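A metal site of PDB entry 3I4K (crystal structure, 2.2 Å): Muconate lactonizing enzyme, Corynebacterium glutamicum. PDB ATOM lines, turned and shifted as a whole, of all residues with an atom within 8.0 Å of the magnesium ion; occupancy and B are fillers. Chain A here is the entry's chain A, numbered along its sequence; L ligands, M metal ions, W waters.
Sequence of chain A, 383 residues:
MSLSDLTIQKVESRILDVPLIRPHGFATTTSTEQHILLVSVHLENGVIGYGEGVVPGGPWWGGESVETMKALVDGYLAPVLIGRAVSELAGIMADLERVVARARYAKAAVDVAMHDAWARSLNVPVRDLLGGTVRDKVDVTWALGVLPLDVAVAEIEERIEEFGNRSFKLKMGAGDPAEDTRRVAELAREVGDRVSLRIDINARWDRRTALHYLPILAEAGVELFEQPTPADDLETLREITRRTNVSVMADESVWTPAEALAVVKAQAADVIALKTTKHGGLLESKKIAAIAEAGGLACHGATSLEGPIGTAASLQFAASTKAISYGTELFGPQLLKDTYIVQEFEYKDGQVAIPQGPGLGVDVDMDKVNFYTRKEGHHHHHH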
ATOM      1  N   PHE A  26       9.671  -2.045  -2.001  1.00  0.00           N
ATOM      2  CA  PHE A  26      10.467  -2.036  -0.781  1.00  0.00           C
ATOM      3  C   PHE A  26      10.094  -0.805   0.041  1.00  0.00           C
ATOM      4  O   PHE A  26       9.161  -0.065  -0.286  1.00  0.00           O
ATOM      5  CB  PHE A  26      11.955  -1.979  -1.118  1.00  0.00           C
ATOM      6  CG  PHE A  26      12.447  -3.149  -1.921  1.00  0.00           C
ATOM      7  CD1 PHE A  26      12.908  -4.306  -1.283  1.00  0.00           C
ATOM      8  CD2 PHE A  26      12.453  -3.108  -3.316  1.00  0.00           C
ATOM      9  CE1 PHE A  26      13.369  -5.388  -2.024  1.00  0.00           C
ATOM     10  CE2 PHE A  26      12.914  -4.190  -4.057  1.00  0.00           C
ATOM     11  CZ  PHE A  26      13.377  -5.326  -3.412  1.00  0.00           C
ATOM     12  N   PRO A  56      19.362  -6.210  -4.291  1.00  0.00           N
ATOM     13  CA  PRO A  56      17.891  -6.146  -4.302  1.00  0.00           C
ATOM     14  C   PRO A  56      17.302  -4.890  -4.926  1.00  0.00           C
ATOM     15  O   PRO A  56      16.909  -3.965  -4.216  1.00  0.00           O
ATOM     16  CB  PRO A  56      17.527  -6.238  -2.811  1.00  0.00           C
ATOM     17  CG  PRO A  56      18.725  -6.877  -2.191  1.00  0.00           C
ATOM     18  CD  PRO A  56      19.862  -6.229  -2.904  1.00  0.00           C
ATOM     19  N   TRP A  60      19.974   1.443  -3.300  1.00  0.00           N
ATOM     20  CA  TRP A  60      19.323   1.893  -2.069  1.00  0.00           C
ATOM     21  C   TRP A  60      19.605   0.894  -0.938  1.00  0.00           C
ATOM     22  O   TRP A  60      19.614   1.247   0.234  1.00  0.00           O
ATOM     23  CB  TRP A  60      17.804   1.979  -2.252  1.00  0.00           C
ATOM     24  CG  TRP A  60      17.167   0.639  -2.501  1.00  0.00           C
ATOM     25  CD1 TRP A  60      17.043  -0.005  -3.696  1.00  0.00           C
ATOM     26  CD2 TRP A  60      16.686  -0.276  -1.502  1.00  0.00           C
ATOM     27  NE1 TRP A  60      16.527  -1.274  -3.509  1.00  0.00           N
ATOM     28  CE2 TRP A  60      16.299  -1.460  -2.171  1.00  0.00           C
ATOM     29  CE3 TRP A  60      16.551  -0.209  -0.103  1.00  0.00           C
ATOM     30  CZ2 TRP A  60      15.792  -2.569  -1.491  1.00  0.00           C
ATOM     31  CZ3 TRP A  60      16.043  -1.318   0.577  1.00  0.00           C
ATOM     32  CH2 TRP A  60      15.670  -2.488  -0.129  1.00  0.00           C
ATOM     33  N   TRP A  61      19.835  -0.363  -1.311  1.00  0.00           N
ATOM     34  CA  TRP A  61      20.079  -1.401  -0.311  1.00  0.00           C
ATOM     35  C   TRP A  61      21.431  -1.224   0.399  1.00  0.00           C
ATOM     36  O   TRP A  61      21.480  -1.161   1.623  1.00  0.00           O
ATOM     37  CB  TRP A  61      20.021  -2.793  -0.964  1.00  0.00           C
ATOM     38  CG  TRP A  61      19.839  -3.905   0.047  1.00  0.00           C
ATOM     39  CD1 TRP A  61      18.663  -4.512   0.404  1.00  0.00           C
ATOM     40  CD2 TRP A  61      20.859  -4.506   0.864  1.00  0.00           C
ATOM     41  NE1 TRP A  61      18.883  -5.450   1.377  1.00  0.00           N
ATOM     42  CE2 TRP A  61      20.212  -5.469   1.684  1.00  0.00           C
ATOM     43  CE3 TRP A  61      22.237  -4.326   0.984  1.00  0.00           C
ATOM     44  CZ2 TRP A  61      20.925  -6.245   2.613  1.00  0.00           C
ATOM     45  CZ3 TRP A  61      22.938  -5.103   1.905  1.00  0.00           C
ATOM     46  CH2 TRP A  61      22.276  -6.044   2.708  1.00  0.00           C
ATOM     47  N   LYS A 169       7.583 -14.003   4.380  1.00  0.00           N
ATOM     48  CA  LYS A 169       8.290 -12.801   4.835  1.00  0.00           C
ATOM     49  C   LYS A 169       7.611 -11.567   4.208  1.00  0.00           C
ATOM     50  O   LYS A 169       7.465 -11.473   2.983  1.00  0.00           O
ATOM     51  CB  LYS A 169       9.742 -12.895   4.390  1.00  0.00           C
ATOM     52  CG  LYS A 169      10.581 -11.648   4.564  1.00  0.00           C
ATOM     53  CD  LYS A 169      11.965 -11.904   3.999  1.00  0.00           C
ATOM     54  CE  LYS A 169      12.718 -10.628   3.737  1.00  0.00           C
ATOM     55  NZ  LYS A 169      14.110 -10.946   3.320  1.00  0.00           N
ATOM     56  N   LYS A 171       7.758  -7.572   3.604  1.00  0.00           N
ATOM     57  CA  LYS A 171       8.584  -6.376   3.600  1.00  0.00           C
ATOM     58  C   LYS A 171       7.736  -5.217   4.146  1.00  0.00           C
ATOM     59  O   LYS A 171       6.528  -5.171   3.947  1.00  0.00           O
ATOM     60  CB  LYS A 171       9.059  -6.070   2.171  1.00  0.00           C
ATOM     61  CG  LYS A 171      10.159  -7.017   1.656  1.00  0.00           C
ATOM     62  CD  LYS A 171      10.395  -6.871   0.144  1.00  0.00           C
ATOM     63  CE  LYS A 171      11.694  -7.536  -0.332  1.00  0.00           C
ATOM     64  NZ  LYS A 171      11.788  -9.017  -0.167  1.00  0.00           N
ATOM     65  N   ILE A 199       8.991 -10.439   9.137  1.00  0.00           N
ATOM     66  CA  ILE A 199       8.963  -9.148   8.471  1.00  0.00           C
ATOM     67  C   ILE A 199      10.391  -8.696   8.190  1.00  0.00           C
ATOM     68  O   ILE A 199      11.358  -9.317   8.653  1.00  0.00           O
ATOM     69  CB  ILE A 199       8.218  -8.074   9.294  1.00  0.00           C
ATOM     70  CG1 ILE A 199       8.860  -7.895  10.675  1.00  0.00           C
ATOM     71  CG2 ILE A 199       6.756  -8.446   9.426  1.00  0.00           C
ATOM     72  CD1 ILE A 199      10.001  -6.899  10.668  1.00  0.00           C
ATOM     73  N   ASP A 200      10.529  -7.642   7.393  1.00  0.00           N
ATOM     74  CA  ASP A 200      11.838  -7.091   7.035  1.00  0.00           C
ATOM     75  C   ASP A 200      11.596  -5.636   6.659  1.00  0.00           C
ATOM     76  O   ASP A 200      10.856  -5.347   5.716  1.00  0.00           O
ATOM     77  CB  ASP A 200      12.431  -7.876   5.855  1.00  0.00           C
ATOM     78  CG  ASP A 200      13.824  -7.411   5.483  1.00  0.00           C
ATOM     79  OD1 ASP A 200      14.316  -6.466   6.126  1.00  0.00           O
ATOM     80  OD2 ASP A 200      14.437  -7.971   4.541  1.00  0.00           O
ATOM     81  N   ILE A 201      12.219  -4.718   7.404  1.00  0.00           N
ATOM     82  CA  ILE A 201      12.050  -3.296   7.152  1.00  0.00           C
ATOM     83  C   ILE A 201      13.255  -2.669   6.466  1.00  0.00           C
ATOM     84  O   ILE A 201      13.323  -1.454   6.281  1.00  0.00           O
ATOM     85  CB  ILE A 201      11.766  -2.548   8.461  1.00  0.00           C
ATOM     86  CG1 ILE A 201      10.890  -3.429   9.359  1.00  0.00           C
ATOM     87  CG2 ILE A 201      11.000  -1.242   8.160  1.00  0.00           C
ATOM     88  CD1 ILE A 201      10.489  -2.786  10.652  1.00  0.00           C
ATOM     89  N   ASN A 202      14.216  -3.505   6.083  1.00  0.00           N
ATOM     90  CA  ASN A 202      15.411  -3.020   5.418  1.00  0.00           C
ATOM     91  C   ASN A 202      16.037  -1.794   6.081  1.00  0.00           C
ATOM     92  O   ASN A 202      16.375  -0.818   5.417  1.00  0.00           O
ATOM     93  CB  ASN A 202      15.096  -2.727   3.949  1.00  0.00           C
ATOM     94  CG  ASN A 202      15.098  -3.979   3.089  1.00  0.00           C
ATOM     95  OD1 ASN A 202      16.151  -4.581   2.858  1.00  0.00           O
ATOM     96  ND2 ASN A 202      13.921  -4.392   2.630  1.00  0.00           N
ATOM     97  N   ALA A 203      16.186  -1.857   7.401  1.00  0.00           N
ATOM     98  CA  ALA A 203      16.803  -0.801   8.188  1.00  0.00           C
ATOM     99  C   ALA A 203      16.169   0.580   8.039  1.00  0.00           C
ATOM    100  O   ALA A 203      16.799   1.566   8.380  1.00  0.00           O
ATOM    101  CB  ALA A 203      18.294  -0.699   7.840  1.00  0.00           C
ATOM    102  N   GLU A 226      13.385  -9.104  10.827  1.00  0.00           N
ATOM    103  CA  GLU A 226      14.616  -8.945  10.045  1.00  0.00           C
ATOM    104  C   GLU A 226      14.966  -7.458   9.914  1.00  0.00           C
ATOM    105  O   GLU A 226      14.097  -6.639   9.611  1.00  0.00           O
ATOM    106  CB  GLU A 226      14.452  -9.554   8.651  1.00  0.00           C
ATOM    107  CG  GLU A 226      15.651  -9.300   7.713  1.00  0.00           C
ATOM    108  CD  GLU A 226      15.549 -10.054   6.396  1.00  0.00           C
ATOM    109  OE1 GLU A 226      14.548 -10.767   6.185  1.00  0.00           O
ATOM    110  OE2 GLU A 226      16.476  -9.940   5.565  1.00  0.00           O
ATOM    111  N   GLN A 227      16.243  -7.144  10.158  1.00  0.00           N
ATOM    112  CA  GLN A 227      16.802  -5.804  10.089  1.00  0.00           C
ATOM    113  C   GLN A 227      15.774  -4.665  10.113  1.00  0.00           C
ATOM    114  O   GLN A 227      15.634  -3.922   9.133  1.00  0.00           O
ATOM    115  CB  GLN A 227      17.673  -5.665   8.839  1.00  0.00           C
ATOM    116  CG  GLN A 227      18.702  -4.548   8.923  1.00  0.00           C
ATOM    117  CD  GLN A 227      19.891  -4.894   9.826  1.00  0.00           C
ATOM    118  OE1 GLN A 227      20.469  -5.989   9.716  1.00  0.00           O
ATOM    119  NE2 GLN A 227      20.270  -3.977  10.705  1.00  0.00           N
ATOM    120  N   MET A 249      16.714 -11.068  12.868  1.00  0.00           N
ATOM    121  CA  MET A 249      17.620 -11.606  11.853  1.00  0.00           C
ATOM    122  C   MET A 249      18.406 -10.430  11.296  1.00  0.00           C
ATOM    123  O   MET A 249      17.830  -9.423  10.876  1.00  0.00           O
ATOM    124  CB  MET A 249      16.856 -12.330  10.723  1.00  0.00           C
ATOM    125  CG  MET A 249      17.748 -12.716   9.530  1.00  0.00           C
ATOM    126  SD  MET A 249      17.106 -14.236   8.505  1.00  0.00           S
ATOM    127  CE  MET A 249      15.756 -13.318   7.442  1.00  0.00           C
ATOM    128  N   ALA A 250      19.733 -10.541  11.312  1.00  0.00           N
ATOM    129  CA  ALA A 250      20.592  -9.477  10.812  1.00  0.00           C
ATOM    130  C   ALA A 250      20.818  -9.675   9.319  1.00  0.00           C
ATOM    131  O   ALA A 250      21.098 -10.784   8.880  1.00  0.00           O
ATOM    132  CB  ALA A 250      21.935  -9.479  11.558  1.00  0.00           C
ATOM    133  N   ASP A 251      20.683  -8.592   8.559  1.00  0.00           N
ATOM    134  CA  ASP A 251      20.897  -8.640   7.118  1.00  0.00           C
ATOM    135  C   ASP A 251      21.903  -7.559   6.741  1.00  0.00           C
ATOM    136  O   ASP A 251      23.073  -7.846   6.577  1.00  0.00           O
ATOM    137  CB  ASP A 251      19.566  -8.434   6.381  1.00  0.00           C
ATOM    138  CG  ASP A 251      19.679  -8.694   4.885  1.00  0.00           C
ATOM    139  OD1 ASP A 251      20.810  -8.930   4.392  1.00  0.00           O
ATOM    140  OD2 ASP A 251      18.628  -8.673   4.199  1.00  0.00           O
ATOM    141  N   GLU A 252      21.466  -6.297   6.642  1.00  0.00           N
ATOM    142  CA  GLU A 252      22.433  -5.254   6.279  1.00  0.00           C
ATOM    143  C   GLU A 252      23.522  -5.100   7.323  1.00  0.00           C
ATOM    144  O   GLU A 252      24.584  -4.576   7.018  1.00  0.00           O
ATOM    145  CB  GLU A 252      21.754  -3.901   6.009  1.00  0.00           C
ATOM    146  CG  GLU A 252      20.308  -3.751   6.424  1.00  0.00           C
ATOM    147  CD  GLU A 252      19.327  -4.413   5.472  1.00  0.00           C
ATOM    148  OE1 GLU A 252      18.816  -3.760   4.535  1.00  0.00           O
ATOM    149  OE2 GLU A 252      19.049  -5.600   5.675  1.00  0.00           O
ATOM    150  N   ALA A 273      21.194 -13.514   7.992  1.00  0.00           N
ATOM    151  CA  ALA A 273      20.757 -13.693   6.598  1.00  0.00           C
ATOM    152  C   ALA A 273      22.020 -13.832   5.764  1.00  0.00           C
ATOM    153  O   ALA A 273      22.662 -12.840   5.422  1.00  0.00           O
ATOM    154  CB  ALA A 273      19.940 -12.483   6.143  1.00  0.00           C
ATOM    155  N   LYS A 275      23.973 -14.516   2.439  1.00  0.00           N
ATOM    156  CA  LYS A 275      23.792 -14.421   0.997  1.00  0.00           C
ATOM    157  C   LYS A 275      25.166 -14.459   0.357  1.00  0.00           C
ATOM    158  O   LYS A 275      26.036 -13.644   0.666  1.00  0.00           O
ATOM    159  CB  LYS A 275      23.110 -13.094   0.646  1.00  0.00           C
ATOM    160  CG  LYS A 275      21.864 -12.786   1.434  1.00  0.00           C
ATOM    161  CD  LYS A 275      21.263 -11.436   1.008  1.00  0.00           C
ATOM    162  CE  LYS A 275      20.013 -11.104   1.823  1.00  0.00           C
ATOM    163  NZ  LYS A 275      19.518  -9.729   1.568  1.00  0.00           N
ATOM    164  N   LYS A 278      26.072 -10.944  -1.162  1.00  0.00           N
ATOM    165  CA  LYS A 278      26.415  -9.907  -0.204  1.00  0.00           C
ATOM    166  C   LYS A 278      27.728 -10.145   0.538  1.00  0.00           C
ATOM    167  O   LYS A 278      28.411  -9.196   0.905  1.00  0.00           O
ATOM    168  CB  LYS A 278      25.282  -9.750   0.827  1.00  0.00           C
ATOM    169  CG  LYS A 278      25.577  -8.782   1.980  1.00  0.00           C
ATOM    170  CD  LYS A 278      24.472  -8.813   3.044  1.00  0.00           C
ATOM    171  CE  LYS A 278      24.242 -10.226   3.587  1.00  0.00           C
ATOM    172  NZ  LYS A 278      23.278 -10.251   4.732  1.00  0.00           N
ATOM    173  N   ALA A 302      19.546 -16.711   2.719  1.00  0.00           N
ATOM    174  CA  ALA A 302      18.941 -15.475   2.225  1.00  0.00           C
ATOM    175  C   ALA A 302      19.252 -15.143   0.770  1.00  0.00           C
ATOM    176  O   ALA A 302      20.233 -15.615   0.184  1.00  0.00           O
ATOM    177  CB  ALA A 302      19.346 -14.297   3.136  1.00  0.00           C
ATOM    178  N   THR A 303      18.417 -14.289   0.194  1.00  0.00           N
ATOM    179  CA  THR A 303      18.561 -13.892  -1.197  1.00  0.00           C
ATOM    180  C   THR A 303      18.632 -12.392  -1.408  1.00  0.00           C
ATOM    181  O   THR A 303      18.030 -11.616  -0.662  1.00  0.00           O
ATOM    182  CB  THR A 303      17.386 -14.440  -2.051  1.00  0.00           C
ATOM    183  OG1 THR A 303      17.620 -14.154  -3.422  1.00  0.00           O
ATOM    184  CG2 THR A 303      16.074 -13.800  -1.627  1.00  0.00           C
ATOM    185  N   SER A 304      19.385 -12.008  -2.420  1.00  0.00           N
ATOM    186  CA  SER A 304      19.516 -10.612  -2.800  1.00  0.00           C
ATOM    187  C   SER A 304      18.674 -10.492  -4.069  1.00  0.00           C
ATOM    188  O   SER A 304      18.868  -9.591  -4.892  1.00  0.00           O
ATOM    189  CB  SER A 304      20.981 -10.279  -3.122  1.00  0.00           C
ATOM    190  OG  SER A 304      21.760 -10.280  -1.952  1.00  0.00           O
ATOM    191  N   GLU A 329      15.243 -18.513   1.448  1.00  0.00           N
ATOM    192  CA  GLU A 329      14.244 -17.675   0.787  1.00  0.00           C
ATOM    193  C   GLU A 329      14.763 -17.522  -0.639  1.00  0.00           C
ATOM    194  O   GLU A 329      14.666 -16.467  -1.248  1.00  0.00           O
ATOM    195  CB  GLU A 329      14.134 -16.292   1.450  1.00  0.00           C
ATOM    196  CG  GLU A 329      15.475 -15.604   1.680  1.00  0.00           C
ATOM    197  CD  GLU A 329      15.338 -14.120   1.987  1.00  0.00           C
ATOM    198  OE1 GLU A 329      14.287 -13.693   2.504  1.00  0.00           O
ATOM    199  OE2 GLU A 329      16.311 -13.376   1.701  1.00  0.00           O
HETATM  200  C1  LIG L   1      16.524  -8.345   1.499  1.00  0.00           C
HETATM  201  O1  LIG L   1      16.852  -7.307   2.058  1.00  0.00           O
HETATM  202  O2  LIG L   1      16.255  -9.434   2.228  1.00  0.00           O
HETATM  203  C2  LIG L   1      16.425  -8.423  -0.005  1.00  0.00           C
HETATM  204 MG    MG M   1      16.634  -8.335   4.135  1.00  0.00          MG
HETATM  205  O   HOH W   1      16.916  -6.724   5.435  1.00  0.00           O
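The side-chain carboxylate (OD1) of Asp 251 is in salt-bridge range of the side-chain amino group (NZ) of Lys 278 (2.8 Å).
N of Asn 202 lies within hydrogen-bond range of O of Gln 227 (3.4 Å).
OD2 of Asp 200 lies close to NZ of Lys 169, 3.2 Å away.
N of Ile 201 lies within hydrogen-bond range of O of Glu 226 (3.5 Å).
The side-chain carboxylate of Asp 200 is in hydrogen-bond range of the backbone NH of Asn 202 (3.0 Å).
N of Glu 252 lies within hydrogen-bond range of OE1 of Gln 227 (3.2 Å).
The side-chain carboxylate of Glu 329 lies within salt-bridge range of the side-chain amino group of Lys 169 (2.9 Å).
The side-chain carboxylate (OE1) of Glu 252 sits close to the side-chain amide oxygen (OD1) of Asn 202, 3.3 Å away.
Residues that only touch the magnesium ion: Lys 169 (3.7 Å), Glu 252 (3.96 Å) and Asn 202 (3.99 Å).
Within 4 Å of the magnesium ion: Lys 169, Asp 200, Asn 202, Glu 226, Asp 251 and Glu 252.
The magnesium ion is bound by OD2 of Asp 251 (2.0 Å).
The magnesium ion is bound by water W1.
The magnesium ion is bound by OE2 of Glu 226, 2.2 Å away.
O2 of the ligand is bound to the magnesium ion, at 2.2 Å.
OD2 of Asp 200 binds the magnesium ion (2.3 Å).
O1 of the ligand is bound to the magnesium ion, at 2.3 Å.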
